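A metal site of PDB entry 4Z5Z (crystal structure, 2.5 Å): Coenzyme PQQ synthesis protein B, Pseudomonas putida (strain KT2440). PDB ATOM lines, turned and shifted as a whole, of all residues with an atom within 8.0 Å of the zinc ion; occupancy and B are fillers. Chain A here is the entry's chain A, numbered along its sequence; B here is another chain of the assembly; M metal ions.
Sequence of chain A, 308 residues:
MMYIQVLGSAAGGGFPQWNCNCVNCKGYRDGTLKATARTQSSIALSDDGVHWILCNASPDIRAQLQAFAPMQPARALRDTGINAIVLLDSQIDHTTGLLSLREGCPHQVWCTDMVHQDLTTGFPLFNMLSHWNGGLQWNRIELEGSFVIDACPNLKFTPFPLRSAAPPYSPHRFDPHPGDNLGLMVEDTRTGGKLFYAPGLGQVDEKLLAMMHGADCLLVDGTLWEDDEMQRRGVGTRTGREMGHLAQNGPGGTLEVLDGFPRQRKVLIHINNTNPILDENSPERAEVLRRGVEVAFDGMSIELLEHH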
ATOM      1  N   GLY A  14      29.020 -28.491 -22.176  1.00  0.00           N
ATOM      2  CA  GLY A  14      29.335 -29.701 -21.438  1.00  0.00           C
ATOM      3  C   GLY A  14      28.092 -30.388 -20.895  1.00  0.00           C
ATOM      4  O   GLY A  14      26.978 -30.001 -21.231  1.00  0.00           O
ATOM      5  N   PHE A  15      28.294 -31.401 -20.059  1.00  0.00           N
ATOM      6  CA  PHE A  15      27.189 -32.075 -19.394  1.00  0.00           C
ATOM      7  C   PHE A  15      27.537 -32.427 -17.958  1.00  0.00           C
ATOM      8  O   PHE A  15      28.478 -33.184 -17.718  1.00  0.00           O
ATOM      9  CB  PHE A  15      26.741 -33.326 -20.160  1.00  0.00           C
ATOM     10  CG  PHE A  15      25.706 -34.141 -19.419  1.00  0.00           C
ATOM     11  CD1 PHE A  15      24.452 -33.611 -19.160  1.00  0.00           C
ATOM     12  CD2 PHE A  15      25.990 -35.423 -19.004  1.00  0.00           C
ATOM     13  CE1 PHE A  15      23.499 -34.359 -18.479  1.00  0.00           C
ATOM     14  CE2 PHE A  15      25.041 -36.185 -18.327  1.00  0.00           C
ATOM     15  CZ  PHE A  15      23.797 -35.645 -18.064  1.00  0.00           C
ATOM     16  N   PRO A  16      26.779 -31.887 -16.988  1.00  0.00           N
ATOM     17  CA  PRO A  16      25.669 -30.944 -17.223  1.00  0.00           C
ATOM     18  C   PRO A  16      26.152 -29.529 -17.530  1.00  0.00           C
ATOM     19  O   PRO A  16      27.250 -29.150 -17.120  1.00  0.00           O
ATOM     20  CB  PRO A  16      24.917 -30.969 -15.888  1.00  0.00           C
ATOM     21  CG  PRO A  16      25.982 -31.263 -14.877  1.00  0.00           C
ATOM     22  CD  PRO A  16      26.908 -32.232 -15.563  1.00  0.00           C
ATOM     23  N   GLN A  17      25.334 -28.770 -18.255  1.00  0.00           N
ATOM     24  CA  GLN A  17      25.641 -27.368 -18.544  1.00  0.00           C
ATOM     25  C   GLN A  17      25.419 -26.538 -17.282  1.00  0.00           C
ATOM     26  O   GLN A  17      24.523 -26.825 -16.492  1.00  0.00           O
ATOM     27  CB  GLN A  17      24.766 -26.858 -19.693  1.00  0.00           C
ATOM     28  CG  GLN A  17      25.226 -25.547 -20.314  1.00  0.00           C
ATOM     29  CD  GLN A  17      24.487 -25.212 -21.609  1.00  0.00           C
ATOM     30  OE1 GLN A  17      24.668 -25.865 -22.636  1.00  0.00           O
ATOM     31  NE2 GLN A  17      23.641 -24.186 -21.552  1.00  0.00           N
ATOM     32  N   TRP A  18      26.245 -25.508 -17.103  1.00  0.00           N
ATOM     33  CA  TRP A  18      26.252 -24.712 -15.874  1.00  0.00           C
ATOM     34  C   TRP A  18      24.905 -24.034 -15.562  1.00  0.00           C
ATOM     35  O   TRP A  18      24.525 -23.891 -14.401  1.00  0.00           O
ATOM     36  CB  TRP A  18      27.367 -23.660 -15.930  1.00  0.00           C
ATOM     37  CG  TRP A  18      27.134 -22.585 -16.946  1.00  0.00           C
ATOM     38  CD1 TRP A  18      27.390 -22.657 -18.282  1.00  0.00           C
ATOM     39  CD2 TRP A  18      26.586 -21.276 -16.708  1.00  0.00           C
ATOM     40  NE1 TRP A  18      27.028 -21.477 -18.895  1.00  0.00           N
ATOM     41  CE2 TRP A  18      26.545 -20.614 -17.949  1.00  0.00           C
ATOM     42  CE3 TRP A  18      26.140 -20.617 -15.565  1.00  0.00           C
ATOM     43  CZ2 TRP A  18      26.065 -19.312 -18.071  1.00  0.00           C
ATOM     44  CZ3 TRP A  18      25.668 -19.311 -15.692  1.00  0.00           C
ATOM     45  CH2 TRP A  18      25.627 -18.678 -16.935  1.00  0.00           C
ATOM     46  N   ASN A  19      24.178 -23.621 -16.598  1.00  0.00           N
ATOM     47  CA  ASN A  19      22.945 -22.880 -16.402  1.00  0.00           C
ATOM     48  C   ASN A  19      21.689 -23.628 -16.824  1.00  0.00           C
ATOM     49  O   ASN A  19      20.596 -23.044 -16.854  1.00  0.00           O
ATOM     50  CB  ASN A  19      23.000 -21.539 -17.145  1.00  0.00           C
ATOM     51  CG  ASN A  19      23.137 -21.719 -18.650  1.00  0.00           C
ATOM     52  OD1 ASN A  19      23.554 -22.770 -19.127  1.00  0.00           O
ATOM     53  ND2 ASN A  19      22.780 -20.684 -19.410  1.00  0.00           N
ATOM     54  N   CYS A  20      21.826 -24.910 -17.154  1.00  0.00           N
ATOM     55  CA  CYS A  20      20.689 -25.683 -17.652  1.00  0.00           C
ATOM     56  C   CYS A  20      20.097 -26.620 -16.601  1.00  0.00           C
ATOM     57  O   CYS A  20      20.825 -27.364 -15.943  1.00  0.00           O
ATOM     58  CB  CYS A  20      21.087 -26.481 -18.897  1.00  0.00           C
ATOM     59  SG  CYS A  20      19.692 -27.259 -19.735  1.00  0.00           S
ATOM     60  N   ASN A  21      18.771 -26.579 -16.476  1.00  0.00           N
ATOM     61  CA  ASN A  21      18.068 -27.515 -15.616  1.00  0.00           C
ATOM     62  C   ASN A  21      17.030 -28.315 -16.402  1.00  0.00           C
ATOM     63  O   ASN A  21      15.881 -28.409 -15.989  1.00  0.00           O
ATOM     64  CB  ASN A  21      17.420 -26.797 -14.438  1.00  0.00           C
ATOM     65  CG  ASN A  21      18.428 -26.068 -13.576  1.00  0.00           C
ATOM     66  OD1 ASN A  21      19.222 -26.698 -12.867  1.00  0.00           O
ATOM     67  ND2 ASN A  21      18.404 -24.744 -13.616  1.00  0.00           N
ATOM     68  N   CYS A  22      17.457 -28.869 -17.531  1.00  0.00           N
ATOM     69  CA  CYS A  22      16.604 -29.752 -18.316  1.00  0.00           C
ATOM     70  C   CYS A  22      16.535 -31.119 -17.653  1.00  0.00           C
ATOM     71  O   CYS A  22      17.166 -31.345 -16.619  1.00  0.00           O
ATOM     72  CB  CYS A  22      17.122 -29.883 -19.754  1.00  0.00           C
ATOM     73  SG  CYS A  22      18.639 -30.863 -19.919  1.00  0.00           S
ATOM     74  N   VAL A  23      15.770 -32.045 -18.236  1.00  0.00           N
ATOM     75  CA  VAL A  23      15.568 -33.362 -17.640  1.00  0.00           C
ATOM     76  C   VAL A  23      16.860 -34.153 -17.466  1.00  0.00           C
ATOM     77  O   VAL A  23      16.963 -34.987 -16.561  1.00  0.00           O
ATOM     78  CB  VAL A  23      14.549 -34.198 -18.443  1.00  0.00           C
ATOM     79  CG1 VAL A  23      13.180 -33.537 -18.420  1.00  0.00           C
ATOM     80  CG2 VAL A  23      15.019 -34.382 -19.878  1.00  0.00           C
ATOM     81  N   ASN A  24      17.846 -33.896 -18.320  1.00  0.00           N
ATOM     82  CA  ASN A  24      19.145 -34.563 -18.218  1.00  0.00           C
ATOM     83  C   ASN A  24      20.044 -33.895 -17.191  1.00  0.00           C
ATOM     84  O   ASN A  24      20.600 -34.552 -16.309  1.00  0.00           O
ATOM     85  CB  ASN A  24      19.846 -34.593 -19.575  1.00  0.00           C
ATOM     86  CG  ASN A  24      19.252 -35.615 -20.528  1.00  0.00           C
ATOM     87  OD1 ASN A  24      18.319 -36.329 -20.187  1.00  0.00           O
ATOM     88  ND2 ASN A  24      19.791 -35.677 -21.740  1.00  0.00           N
ATOM     89  N   CYS A  25      20.189 -32.577 -17.297  1.00  0.00           N
ATOM     90  CA  CYS A  25      21.059 -31.821 -16.406  1.00  0.00           C
ATOM     91  C   CYS A  25      20.552 -31.835 -14.964  1.00  0.00           C
ATOM     92  O   CYS A  25      21.341 -31.936 -14.028  1.00  0.00           O
ATOM     93  CB  CYS A  25      21.238 -30.387 -16.906  1.00  0.00           C
ATOM     94  SG  CYS A  25      22.326 -30.217 -18.350  1.00  0.00           S
ATOM     95  N   LYS A  26      19.234 -31.746 -14.788  1.00  0.00           N
ATOM     96  CA  LYS A  26      18.646 -31.790 -13.455  1.00  0.00           C
ATOM     97  C   LYS A  26      18.598 -33.229 -12.936  1.00  0.00           C
ATOM     98  O   LYS A  26      18.823 -33.479 -11.749  1.00  0.00           O
ATOM     99  CB  LYS A  26      17.251 -31.167 -13.461  1.00  0.00           C
ATOM    100  CG  LYS A  26      16.676 -30.914 -12.075  1.00  0.00           C
ATOM    101  CD  LYS A  26      15.399 -30.091 -12.162  1.00  0.00           C
ATOM    102  CE  LYS A  26      14.763 -29.904 -10.801  1.00  0.00           C
ATOM    103  NZ  LYS A  26      14.423 -31.206 -10.167  1.00  0.00           N
ATOM    104  N   GLY A  27      18.328 -34.159 -13.838  1.00  0.00           N
ATOM    105  CA  GLY A  27      18.299 -35.577 -13.493  1.00  0.00           C
ATOM    106  C   GLY A  27      19.656 -36.069 -13.025  1.00  0.00           C
ATOM    107  O   GLY A  27      19.744 -36.969 -12.195  1.00  0.00           O
ATOM    108  N   ARG A  29      21.958 -33.960 -11.527  1.00  0.00           N
ATOM    109  CA  ARG A  29      22.188 -33.299 -10.241  1.00  0.00           C
ATOM    110  C   ARG A  29      21.343 -33.903  -9.120  1.00  0.00           C
ATOM    111  O   ARG A  29      21.805 -33.990  -7.980  1.00  0.00           O
ATOM    112  CB  ARG A  29      21.908 -31.793 -10.353  1.00  0.00           C
ATOM    113  CG  ARG A  29      22.795 -31.054 -11.344  1.00  0.00           C
ATOM    114  CD  ARG A  29      22.642 -29.542 -11.198  1.00  0.00           C
ATOM    115  NE  ARG A  29      23.375 -28.819 -12.238  1.00  0.00           N
ATOM    116  CZ  ARG A  29      22.818 -28.360 -13.355  1.00  0.00           C
ATOM    117  NH1 ARG A  29      23.557 -27.707 -14.241  1.00  0.00           N
ATOM    118  NH2 ARG A  29      21.525 -28.549 -13.577  1.00  0.00           N
ATOM    119  N   MET A 230      16.015 -28.659 -28.674  1.00  0.00           N
ATOM    120  CA  MET A 230      16.101 -27.516 -27.770  1.00  0.00           C
ATOM    121  C   MET A 230      14.721 -26.990 -27.371  1.00  0.00           C
ATOM    122  O   MET A 230      14.533 -26.531 -26.245  1.00  0.00           O
ATOM    123  CB  MET A 230      16.930 -26.400 -28.416  1.00  0.00           C
ATOM    124  CG  MET A 230      18.372 -26.791 -28.716  1.00  0.00           C
ATOM    125  SD  MET A 230      19.336 -27.051 -27.216  1.00  0.00           S
ATOM    126  CE  MET A 230      19.232 -25.431 -26.472  1.00  0.00           C
ATOM    127  N   ARG A 233      12.944 -29.525 -24.943  1.00  0.00           N
ATOM    128  CA  ARG A 233      13.482 -29.420 -23.596  1.00  0.00           C
ATOM    129  C   ARG A 233      13.076 -28.080 -22.996  1.00  0.00           C
ATOM    130  O   ARG A 233      13.120 -27.886 -21.780  1.00  0.00           O
ATOM    131  CB  ARG A 233      15.000 -29.562 -23.605  1.00  0.00           C
ATOM    132  CG  ARG A 233      15.491 -30.874 -24.210  1.00  0.00           C
ATOM    133  CD  ARG A 233      14.898 -32.069 -23.502  1.00  0.00           C
ATOM    134  NE  ARG A 233      15.660 -33.295 -23.744  1.00  0.00           N
ATOM    135  CZ  ARG A 233      15.226 -34.515 -23.469  1.00  0.00           C
ATOM    136  NH1 ARG A 233      15.988 -35.571 -23.738  1.00  0.00           N
ATOM    137  NH2 ARG A 233      14.025 -34.691 -22.942  1.00  0.00           N
ATOM    138  N   VAL A 235      14.562 -25.112 -23.519  1.00  0.00           N
ATOM    139  CA  VAL A 235      15.738 -24.364 -23.102  1.00  0.00           C
ATOM    140  C   VAL A 235      16.338 -23.541 -24.248  1.00  0.00           C
ATOM    141  O   VAL A 235      17.298 -22.794 -24.043  1.00  0.00           O
ATOM    142  CB  VAL A 235      16.824 -25.287 -22.529  1.00  0.00           C
ATOM    143  CG1 VAL A 235      16.356 -25.935 -21.242  1.00  0.00           C
ATOM    144  CG2 VAL A 235      17.204 -26.351 -23.552  1.00  0.00           C
ATOM    145  N   ASN A 272      25.146 -32.989 -27.015  1.00  0.00           N
ATOM    146  CA  ASN A 272      24.584 -31.909 -26.201  1.00  0.00           C
ATOM    147  C   ASN A 272      23.898 -32.415 -24.940  1.00  0.00           C
ATOM    148  O   ASN A 272      23.392 -33.538 -24.900  1.00  0.00           O
ATOM    149  CB  ASN A 272      23.611 -31.061 -27.016  1.00  0.00           C
ATOM    150  CG  ASN A 272      23.337 -29.695 -26.393  1.00  0.00           C
ATOM    151  OD1 ASN A 272      24.262 -28.961 -26.053  1.00  0.00           O
ATOM    152  ND2 ASN A 272      22.058 -29.366 -26.230  1.00  0.00           N
ATOM    153  N   ASN A 273      23.864 -31.563 -23.910  1.00  0.00           N
ATOM    154  CA  ASN A 273      23.305 -31.912 -22.610  1.00  0.00           C
ATOM    155  C   ASN A 273      21.821 -32.278 -22.646  1.00  0.00           C
ATOM    156  O   ASN A 273      21.287 -32.830 -21.685  1.00  0.00           O
ATOM    157  CB  ASN A 273      23.510 -30.755 -21.632  1.00  0.00           C
ATOM    158  CG  ASN A 273      22.652 -29.550 -21.992  1.00  0.00           C
ATOM    159  OD1 ASN A 273      21.504 -29.429 -21.550  1.00  0.00           O
ATOM    160  ND2 ASN A 273      23.199 -28.648 -22.799  1.00  0.00           N
ATOM    161  N   THR A 274      21.152 -31.936 -23.747  1.00  0.00           N
ATOM    162  CA  THR A 274      19.718 -32.201 -23.887  1.00  0.00           C
ATOM    163  C   THR A 274      19.424 -33.545 -24.570  1.00  0.00           C
ATOM    164  O   THR A 274      18.278 -33.992 -24.608  1.00  0.00           O
ATOM    165  CB  THR A 274      19.021 -31.075 -24.678  1.00  0.00           C
ATOM    166  OG1 THR A 274      19.655 -30.919 -25.954  1.00  0.00           O
ATOM    167  CG2 THR A 274      19.070 -29.754 -23.913  1.00  0.00           C
ATOM    168  N   ASN A 275      20.467 -34.188 -25.099  1.00  0.00           N
ATOM    169  CA  ASN A 275      20.330 -35.423 -25.855  1.00  0.00           C
ATOM    170  C   ASN A 275      20.052 -36.622 -24.944  1.00  0.00           C
ATOM    171  O   ASN A 275      20.831 -36.917 -24.037  1.00  0.00           O
ATOM    172  CB  ASN A 275      21.598 -35.665 -26.685  1.00  0.00           C
ATOM    173  CG  ASN A 275      21.380 -36.652 -27.829  1.00  0.00           C
ATOM    174  OD1 ASN A 275      20.593 -37.596 -27.723  1.00  0.00           O
ATOM    175  ND2 ASN A 275      22.101 -36.440 -28.926  1.00  0.00           N
ATOM    176  N   LEU A 278      22.367 -39.664 -23.656  1.00  0.00           N
ATOM    177  CA  LEU A 278      23.196 -39.562 -22.461  1.00  0.00           C
ATOM    178  C   LEU A 278      22.574 -40.356 -21.305  1.00  0.00           C
ATOM    179  O   LEU A 278      23.282 -40.802 -20.406  1.00  0.00           O
ATOM    180  CB  LEU A 278      23.384 -38.093 -22.064  1.00  0.00           C
ATOM    181  CG  LEU A 278      24.154 -37.227 -23.055  1.00  0.00           C
ATOM    182  CD1 LEU A 278      24.334 -35.808 -22.528  1.00  0.00           C
ATOM    183  CD2 LEU A 278      25.495 -37.853 -23.394  1.00  0.00           C
ATOM    184  N   LEU B  77      14.290 -23.508 -16.111  1.00  0.00           N
ATOM    185  CA  LEU B  77      15.065 -24.401 -16.970  1.00  0.00           C
ATOM    186  C   LEU B  77      16.421 -23.790 -17.279  1.00  0.00           C
ATOM    187  O   LEU B  77      17.413 -24.513 -17.452  1.00  0.00           O
ATOM    188  CB  LEU B  77      14.297 -24.711 -18.254  1.00  0.00           C
ATOM    189  CG  LEU B  77      13.008 -25.503 -18.043  1.00  0.00           C
ATOM    190  CD1 LEU B  77      12.296 -25.779 -19.353  1.00  0.00           C
ATOM    191  CD2 LEU B  77      13.310 -26.799 -17.312  1.00  0.00           C
ATOM    192  N   ARG B  78      16.454 -22.468 -17.334  1.00  0.00           N
ATOM    193  CA  ARG B  78      17.702 -21.733 -17.452  1.00  0.00           C
ATOM    194  C   ARG B  78      17.842 -20.832 -16.236  1.00  0.00           C
ATOM    195  O   ARG B  78      17.008 -19.946 -16.011  1.00  0.00           O
ATOM    196  CB  ARG B  78      17.751 -20.910 -18.749  1.00  0.00           C
ATOM    197  CG  ARG B  78      18.018 -21.738 -20.000  1.00  0.00           C
ATOM    198  CD  ARG B  78      19.453 -22.246 -20.003  1.00  0.00           C
ATOM    199  NE  ARG B  78      19.610 -23.530 -20.683  1.00  0.00           N
ATOM    200  CZ  ARG B  78      20.153 -23.670 -21.889  1.00  0.00           C
ATOM    201  NH1 ARG B  78      20.602 -22.619 -22.553  1.00  0.00           N
ATOM    202  NH2 ARG B  78      20.251 -24.880 -22.443  1.00  0.00           N
HETATM  203 ZN    ZN M   1      20.586 -29.467 -19.763  1.00  0.00          ZN
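Four residues have an atom within 4 Å of the zinc ion: Cys 20, Cys 22, Cys 25 and Asn 273. Along chain A the residues within 4 Å of the zinc ion span positions 20 to 273. The nearest printed residue that does not touch the zinc ion is Thr 274 (4.4 Å).
The zinc ion is bound by the side-chain amide oxygen (OD1) of Asn 273 (2.0 Å), the side-chain sulfur (SG) of Cys 25 (2.4 Å), the side-chain sulfur (SG) of Cys 20 (2.4 Å) and the side-chain sulfur (SG) of Cys 22 (2.4 Å).
OE1 of Gln 17 lies within hydrogen-bond range of ND2 of Asn 273, at 3.2 Å. O of Asn 273 lies close to ND2 of Asn 24, 3.2 Å away. OD1 of Asn 272 sits at hydrogen-bond distance from ND2 of Asn 273 (3.4 Å). The side-chain sulfur of Cys 25 sits close to the backbone NH of Gln 17 (3.3 Å). The guanidinium group (NH2) of Arg 29 lies close to the backbone carbonyl oxygen (O) of Cys 25. The guanidinium group (NH2) of Arg 78 of chain B sits close to the side-chain sulfur (SG) of Cys 20. The guanidinium group (NH2) of Arg 29 lies within hydrogen-bond range of the backbone carbonyl oxygen (O) of Cys 20 (2.7 Å). N of Asn 24 sits close to SG of Cys 22 (3.5 Å).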
